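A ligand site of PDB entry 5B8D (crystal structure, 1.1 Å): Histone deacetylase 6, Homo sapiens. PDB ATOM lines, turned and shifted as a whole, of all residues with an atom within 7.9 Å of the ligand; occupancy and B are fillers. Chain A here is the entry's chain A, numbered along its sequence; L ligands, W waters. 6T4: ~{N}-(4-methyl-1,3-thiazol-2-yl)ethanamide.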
ATOM      1  N   GLN A  34       1.019  12.858   2.689  1.00  0.00           N
ATOM      2  CA  GLN A  34       2.274  12.792   1.856  1.00  0.00           C
ATOM      3  C   GLN A  34       2.268  12.501   0.323  1.00  0.00           C
ATOM      4  O   GLN A  34       2.899  13.226  -0.453  1.00  0.00           O
ATOM      5  CB  GLN A  34       3.218  11.767   2.509  1.00  0.00           C
ATOM      6  CG  GLN A  34       3.738  12.221   3.863  1.00  0.00           C
ATOM      7  CD  GLN A  34       5.139  11.736   4.142  1.00  0.00           C
ATOM      8  OE1 GLN A  34       5.863  11.401   3.216  1.00  0.00           O
ATOM      9  NE2 GLN A  34       5.548  11.728   5.406  1.00  0.00           N
ATOM     10  N   GLU A  35       1.617  11.408  -0.103  1.00  0.00           N
ATOM     11  CA  GLU A  35       1.488  10.997  -1.527  1.00  0.00           C
ATOM     12  C   GLU A  35       0.106  10.355  -1.842  1.00  0.00           C
ATOM     13  O   GLU A  35       0.001   9.163  -2.152  1.00  0.00           O
ATOM     14  CB  GLU A  35       2.635  10.001  -1.917  1.00  0.00           C
ATOM     15  CG  GLU A  35       4.030  10.646  -1.930  1.00  0.00           C
ATOM     16  CD  GLU A  35       5.207   9.684  -2.073  1.00  0.00           C
ATOM     17  OE1 GLU A  35       5.043   8.515  -2.531  1.00  0.00           O
ATOM     18  OE2 GLU A  35       6.341  10.109  -1.717  1.00  0.00           O
ATOM     19  N   ASN A  36      -0.955  11.163  -1.844  1.00  0.00           N
ATOM     20  CA  ASN A  36      -2.334  10.667  -1.982  1.00  0.00           C
ATOM     21  C   ASN A  36      -2.851  10.715  -3.431  1.00  0.00           C
ATOM     22  O   ASN A  36      -2.399  11.517  -4.258  1.00  0.00           O
ATOM     23  CB  ASN A  36      -3.281  11.461  -1.048  1.00  0.00           C
ATOM     24  CG  ASN A  36      -2.986  11.172   0.431  1.00  0.00           C
ATOM     25  OD1 ASN A  36      -2.842  10.032   0.832  1.00  0.00           O
ATOM     26  ND2 ASN A  36      -2.877  12.223   1.234  1.00  0.00           N
ATOM     27  N   TRP A  37      -3.794   9.811  -3.678  1.00  0.00           N
ATOM     28  CA  TRP A  37      -4.546   9.668  -4.925  1.00  0.00           C
ATOM     29  C   TRP A  37      -6.030   9.856  -4.630  1.00  0.00           C
ATOM     30  O   TRP A  37      -6.495   9.557  -3.503  1.00  0.00           O
ATOM     31  CB  TRP A  37      -4.326   8.252  -5.515  1.00  0.00           C
ATOM     32  CG  TRP A  37      -2.923   7.861  -5.894  1.00  0.00           C
ATOM     33  CD1 TRP A  37      -1.952   7.386  -5.043  1.00  0.00           C
ATOM     34  CD2 TRP A  37      -2.331   7.831  -7.211  1.00  0.00           C
ATOM     35  NE1 TRP A  37      -0.810   7.089  -5.744  1.00  0.00           N
ATOM     36  CE2 TRP A  37      -1.017   7.349  -7.074  1.00  0.00           C
ATOM     37  CE3 TRP A  37      -2.814   8.123  -8.505  1.00  0.00           C
ATOM     38  CZ2 TRP A  37      -0.149   7.203  -8.177  1.00  0.00           C
ATOM     39  CZ3 TRP A  37      -1.951   7.952  -9.593  1.00  0.00           C
ATOM     40  CH2 TRP A  37      -0.638   7.507  -9.423  1.00  0.00           C
ATOM     41  N   VAL A  38      -6.801  10.281  -5.656  1.00  0.00           N
ATOM     42  CA  VAL A  38      -8.295  10.301  -5.568  1.00  0.00           C
ATOM     43  C   VAL A  38      -8.866   9.259  -6.552  1.00  0.00           C
ATOM     44  O   VAL A  38      -8.435   9.183  -7.730  1.00  0.00           O
ATOM     45  CB  VAL A  38      -8.902  11.743  -5.786  1.00  0.00           C
ATOM     46  CG1 VAL A  38      -8.593  12.355  -7.172  1.00  0.00           C
ATOM     47  CG2 VAL A  38     -10.408  11.770  -5.514  1.00  0.00           C
ATOM     48  N   TYR A  46      -6.937   8.161  -0.816  1.00  0.00           N
ATOM     49  CA  TYR A  46      -6.110   7.156  -0.083  1.00  0.00           C
ATOM     50  C   TYR A  46      -4.644   7.256  -0.554  1.00  0.00           C
ATOM     51  O   TYR A  46      -4.350   7.686  -1.696  1.00  0.00           O
ATOM     52  CB  TYR A  46      -6.637   5.714  -0.300  1.00  0.00           C
ATOM     53  CG  TYR A  46      -8.031   5.452   0.240  1.00  0.00           C
ATOM     54  CD1 TYR A  46      -8.282   5.400   1.625  1.00  0.00           C
ATOM     55  CD2 TYR A  46      -9.109   5.272  -0.633  1.00  0.00           C
ATOM     56  CE1 TYR A  46      -9.582   5.203   2.127  1.00  0.00           C
ATOM     57  CE2 TYR A  46     -10.400   5.050  -0.145  1.00  0.00           C
ATOM     58  CZ  TYR A  46     -10.634   5.013   1.239  1.00  0.00           C
ATOM     59  OH  TYR A  46     -11.916   4.817   1.743  1.00  0.00           O
ATOM     60  N   CYS A  47      -3.724   6.819   0.309  1.00  0.00           N
ATOM     61  CA  CYS A  47      -2.268   6.982   0.066  1.00  0.00           C
ATOM     62  C   CYS A  47      -1.666   5.969  -0.935  1.00  0.00           C
ATOM     63  O   CYS A  47      -2.193   4.850  -1.177  1.00  0.00           O
ATOM     64  CB  CYS A  47      -1.472   6.970   1.409  1.00  0.00           C
ATOM     65  SG  CYS A  47      -1.482   5.376   2.328  1.00  0.00           S
ATOM     66  N   GLY A  48      -0.528   6.370  -1.504  1.00  0.00           N
ATOM     67  CA  GLY A  48       0.178   5.576  -2.515  1.00  0.00           C
ATOM     68  C   GLY A  48       0.964   4.388  -1.960  1.00  0.00           C
ATOM     69  O   GLY A  48       1.155   4.204  -0.722  1.00  0.00           O
ATOM     70  N   ARG A  49       1.474   3.575  -2.888  1.00  0.00           N
ATOM     71  CA  ARG A  49       2.119   2.300  -2.548  1.00  0.00           C
ATOM     72  C   ARG A  49       3.414   2.464  -1.728  1.00  0.00           C
ATOM     73  O   ARG A  49       3.805   1.512  -1.023  1.00  0.00           O
ATOM     74  CB  ARG A  49       2.375   1.456  -3.800  1.00  0.00           C
ATOM     75  CG  ARG A  49       3.472   1.939  -4.727  1.00  0.00           C
ATOM     76  CD  ARG A  49       3.408   1.183  -6.029  1.00  0.00           C
ATOM     77  NE  ARG A  49       4.415   1.583  -6.980  1.00  0.00           N
ATOM     78  CZ  ARG A  49       4.482   1.144  -8.235  1.00  0.00           C
ATOM     79  NH1 ARG A  49       3.560   0.306  -8.720  1.00  0.00           N
ATOM     80  NH2 ARG A  49       5.447   1.589  -9.025  1.00  0.00           N
ATOM     81  N   TYR A  50       4.085   3.617  -1.850  1.00  0.00           N
ATOM     82  CA  TYR A  50       5.339   3.854  -1.104  1.00  0.00           C
ATOM     83  C   TYR A  50       5.088   4.358   0.324  1.00  0.00           C
ATOM     84  O   TYR A  50       6.020   4.365   1.143  1.00  0.00           O
ATOM     85  CB  TYR A  50       6.286   4.811  -1.872  1.00  0.00           C
ATOM     86  CG  TYR A  50       6.656   4.311  -3.271  1.00  0.00           C
ATOM     87  CD1 TYR A  50       7.171   3.036  -3.467  1.00  0.00           C
ATOM     88  CD2 TYR A  50       6.474   5.116  -4.388  1.00  0.00           C
ATOM     89  CE1 TYR A  50       7.470   2.562  -4.742  1.00  0.00           C
ATOM     90  CE2 TYR A  50       6.767   4.661  -5.674  1.00  0.00           C
ATOM     91  CZ  TYR A  50       7.269   3.376  -5.852  1.00  0.00           C
ATOM     92  OH  TYR A  50       7.575   2.868  -7.113  1.00  0.00           O
ATOM     93  N   ILE A  51       3.839   4.737   0.644  1.00  0.00           N
ATOM     94  CA  ILE A  51       3.433   5.151   2.002  1.00  0.00           C
ATOM     95  C   ILE A  51       2.881   3.893   2.705  1.00  0.00           C
ATOM     96  O   ILE A  51       3.679   2.992   3.029  1.00  0.00           O
ATOM     97  CB  ILE A  51       2.487   6.391   1.986  1.00  0.00           C
ATOM     98  CG1 ILE A  51       2.981   7.473   1.002  1.00  0.00           C
ATOM     99  CG2 ILE A  51       2.305   6.930   3.402  1.00  0.00           C
ATOM    100  CD1 ILE A  51       4.363   8.003   1.288  1.00  0.00           C
ATOM    101  N   LEU A  68      -6.315   9.264  -9.744  1.00  0.00           N
ATOM    102  CA  LEU A  68      -5.616  10.512 -10.132  1.00  0.00           C
ATOM    103  C   LEU A  68      -4.637  10.953  -9.024  1.00  0.00           C
ATOM    104  O   LEU A  68      -5.036  11.056  -7.836  1.00  0.00           O
ATOM    105  CB  LEU A  68      -6.671  11.615 -10.416  1.00  0.00           C
ATOM    106  CG  LEU A  68      -6.133  13.007 -10.800  1.00  0.00           C
ATOM    107  CD1 LEU A  68      -5.475  13.024 -12.163  1.00  0.00           C
ATOM    108  CD2 LEU A  68      -7.252  14.031 -10.729  1.00  0.00           C
ATOM    109  N   SER A  69      -3.383  11.244  -9.396  1.00  0.00           N
ATOM    110  CA  SER A  69      -2.344  11.616  -8.410  1.00  0.00           C
ATOM    111  C   SER A  69      -2.468  13.081  -7.995  1.00  0.00           C
ATOM    112  O   SER A  69      -2.481  13.988  -8.847  1.00  0.00           O
ATOM    113  CB  SER A  69      -0.961  11.432  -9.047  1.00  0.00           C
ATOM    114  OG  SER A  69       0.063  12.045  -8.249  1.00  0.00           O
ATOM    115  N   TYR A  70      -2.473  13.327  -6.674  1.00  0.00           N
ATOM    116  CA  TYR A  70      -2.407  14.717  -6.155  1.00  0.00           C
ATOM    117  C   TYR A  70      -0.974  15.284  -6.110  1.00  0.00           C
ATOM    118  O   TYR A  70      -0.808  16.465  -5.767  1.00  0.00           O
ATOM    119  CB  TYR A  70      -3.142  14.820  -4.798  1.00  0.00           C
ATOM    120  CG  TYR A  70      -4.671  14.806  -4.877  1.00  0.00           C
ATOM    121  CD1 TYR A  70      -5.394  15.127  -6.042  1.00  0.00           C
ATOM    122  CD2 TYR A  70      -5.448  14.533  -3.734  1.00  0.00           C
ATOM    123  CE1 TYR A  70      -6.792  15.205  -6.046  1.00  0.00           C
ATOM    124  CE2 TYR A  70      -6.831  14.621  -3.726  1.00  0.00           C
ATOM    125  CZ  TYR A  70      -7.524  14.978  -4.871  1.00  0.00           C
ATOM    126  OH  TYR A  70      -8.911  15.122  -4.951  1.00  0.00           O
ATOM    127  N   ILE A  71       0.041  14.481  -6.480  1.00  0.00           N
ATOM    128  CA  ILE A  71       1.421  14.988  -6.670  1.00  0.00           C
ATOM    129  C   ILE A  71       1.591  15.600  -8.064  1.00  0.00           C
ATOM    130  O   ILE A  71       2.148  16.699  -8.184  1.00  0.00           O
ATOM    131  CB  ILE A  71       2.482  13.868  -6.419  1.00  0.00           C
ATOM    132  CG1 ILE A  71       2.508  13.429  -4.951  1.00  0.00           C
ATOM    133  CG2 ILE A  71       3.892  14.277  -6.882  1.00  0.00           C
ATOM    134  CD1 ILE A  71       3.364  14.265  -4.047  1.00  0.00           C
ATOM    135  N   ASP A  72       1.171  14.876  -9.110  1.00  0.00           N
ATOM    136  CA  ASP A  72       1.510  15.288 -10.501  1.00  0.00           C
ATOM    137  C   ASP A  72       0.376  15.177 -11.517  1.00  0.00           C
ATOM    138  O   ASP A  72       0.622  15.403 -12.724  1.00  0.00           O
ATOM    139  CB  ASP A  72       2.781  14.540 -10.989  1.00  0.00           C
ATOM    140  CG  ASP A  72       2.603  13.041 -10.895  1.00  0.00           C
ATOM    141  OD1 ASP A  72       1.478  12.554 -11.156  1.00  0.00           O
ATOM    142  OD2 ASP A  72       3.554  12.338 -10.459  1.00  0.00           O
ATOM    143  N   LEU A  73      -0.844  14.841 -11.072  1.00  0.00           N
ATOM    144  CA  LEU A  73      -2.040  14.809 -11.957  1.00  0.00           C
ATOM    145  C   LEU A  73      -1.958  13.699 -13.041  1.00  0.00           C
ATOM    146  O   LEU A  73      -2.728  13.756 -14.017  1.00  0.00           O
ATOM    147  CB  LEU A  73      -2.379  16.190 -12.552  1.00  0.00           C
ATOM    148  CG  LEU A  73      -2.483  17.325 -11.537  1.00  0.00           C
ATOM    149  CD1 LEU A  73      -2.850  18.638 -12.241  1.00  0.00           C
ATOM    150  CD2 LEU A  73      -3.426  17.059 -10.374  1.00  0.00           C
ATOM    151  N   SER A  74      -1.107  12.689 -12.851  1.00  0.00           N
ATOM    152  CA  SER A  74      -1.161  11.496 -13.692  1.00  0.00           C
ATOM    153  C   SER A  74      -2.361  10.613 -13.316  1.00  0.00           C
ATOM    154  O   SER A  74      -2.789  10.596 -12.154  1.00  0.00           O
ATOM    155  CB  SER A  74       0.134  10.707 -13.622  1.00  0.00           C
ATOM    156  OG  SER A  74       0.414  10.237 -12.339  1.00  0.00           O
ATOM    157  N   TRP A  76      -3.692   6.640 -13.361  1.00  0.00           N
ATOM    158  CA  TRP A  76      -3.238   5.237 -13.428  1.00  0.00           C
ATOM    159  C   TRP A  76      -4.442   4.290 -13.436  1.00  0.00           C
ATOM    160  O   TRP A  76      -5.380   4.464 -12.620  1.00  0.00           O
ATOM    161  CB  TRP A  76      -2.368   4.939 -12.196  1.00  0.00           C
ATOM    162  CG  TRP A  76      -1.840   3.509 -12.056  1.00  0.00           C
ATOM    163  CD1 TRP A  76      -2.277   2.561 -11.178  1.00  0.00           C
ATOM    164  CD2 TRP A  76      -0.740   2.918 -12.780  1.00  0.00           C
ATOM    165  NE1 TRP A  76      -1.521   1.412 -11.314  1.00  0.00           N
ATOM    166  CE2 TRP A  76      -0.563   1.603 -12.274  1.00  0.00           C
ATOM    167  CE3 TRP A  76       0.124   3.373 -13.784  1.00  0.00           C
ATOM    168  CZ2 TRP A  76       0.442   0.723 -12.761  1.00  0.00           C
ATOM    169  CZ3 TRP A  76       1.136   2.504 -14.282  1.00  0.00           C
ATOM    170  CH2 TRP A  76       1.280   1.202 -13.755  1.00  0.00           C
ATOM    171  N   TYR A  83      -0.436   4.226 -17.337  1.00  0.00           N
ATOM    172  CA  TYR A  83      -1.015   5.573 -17.319  1.00  0.00           C
ATOM    173  C   TYR A  83      -1.899   5.764 -18.567  1.00  0.00           C
ATOM    174  O   TYR A  83      -1.606   5.181 -19.650  1.00  0.00           O
ATOM    175  CB  TYR A  83       0.082   6.641 -17.262  1.00  0.00           C
ATOM    176  CG  TYR A  83       0.975   6.577 -16.010  1.00  0.00           C
ATOM    177  CD1 TYR A  83       0.546   7.072 -14.781  1.00  0.00           C
ATOM    178  CD2 TYR A  83       2.250   6.015 -16.074  1.00  0.00           C
ATOM    179  CE1 TYR A  83       1.399   6.978 -13.659  1.00  0.00           C
ATOM    180  CE2 TYR A  83       3.101   5.933 -14.986  1.00  0.00           C
ATOM    181  CZ  TYR A  83       2.675   6.407 -13.776  1.00  0.00           C
ATOM    182  OH  TYR A  83       3.543   6.340 -12.689  1.00  0.00           O
HETATM  183  C1  6T4 L   1       4.677   9.591 -11.378  1.00  0.00           C
HETATM  184  C2  6T4 L   1       4.278   9.024 -10.035  1.00  0.00           C
HETATM  185  C3  6T4 L   1       2.817   9.416  -8.124  1.00  0.00           C
HETATM  186  C4  6T4 L   1       1.491   9.601  -6.342  1.00  0.00           C
HETATM  187  C5  6T4 L   1       2.214   8.499  -5.969  1.00  0.00           C
HETATM  188  C6  6T4 L   1       0.359  10.229  -5.560  1.00  0.00           C
HETATM  189  O   6T4 L   1       4.737   7.985  -9.594  1.00  0.00           O
HETATM  190  N   6T4 L   1       3.344   9.775  -9.361  1.00  0.00           N
HETATM  191  S   6T4 L   1       3.352   8.052  -7.202  1.00  0.00           S
HETATM  192  N1  6T4 L   1       1.866  10.133  -7.572  1.00  0.00           N
HETATM  193  O   HOH W   1       3.001   5.241  -5.795  1.00  0.00           O
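OG of Ser 69 lies within hydrogen-bond range of N1 of the ligand, 2.7 Å away. The side-chain carboxylate (OD2) of Asp 72 is in hydrogen-bond range of a nitrogen (N) of the ligand, at 2.8 Å.
O of Tyr 46 lies within hydrogen-bond range of N of Trp 37, 3.0 Å away. N of Ser 69 is in hydrogen-bond range of O of Ser 74 (2.9 Å). The side-chain hydroxyl (OG) of Ser 69 is in hydrogen-bond range of the backbone NH (N) of Ile 71, at 3.0 Å. The side-chain carboxylate (OD1) of Asp 72 sits at hydrogen-bond distance from the side-chain hydroxyl (OG) of Ser 74. O of Asn 36 is in hydrogen-bond range of N of Tyr 70 (3.0 Å). The backbone NH (N) of Gly 48 lies within hydrogen-bond range of the backbone carbonyl oxygen (O) of Glu 35, 2.9 Å away. The backbone NH (N) of Asp 72 sits at hydrogen-bond distance from the side-chain hydroxyl (OG) of Ser 69, at 3.2 Å. OD1 of Asn 36 sits close to N of Cys 47 (3.4 Å).
Residues that only touch the ligand: Asn 36, Trp 37, Glu 35, Tyr 83 and Ile 71. Of the 20 residues printed, 7 come within 4 Å of the ligand.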
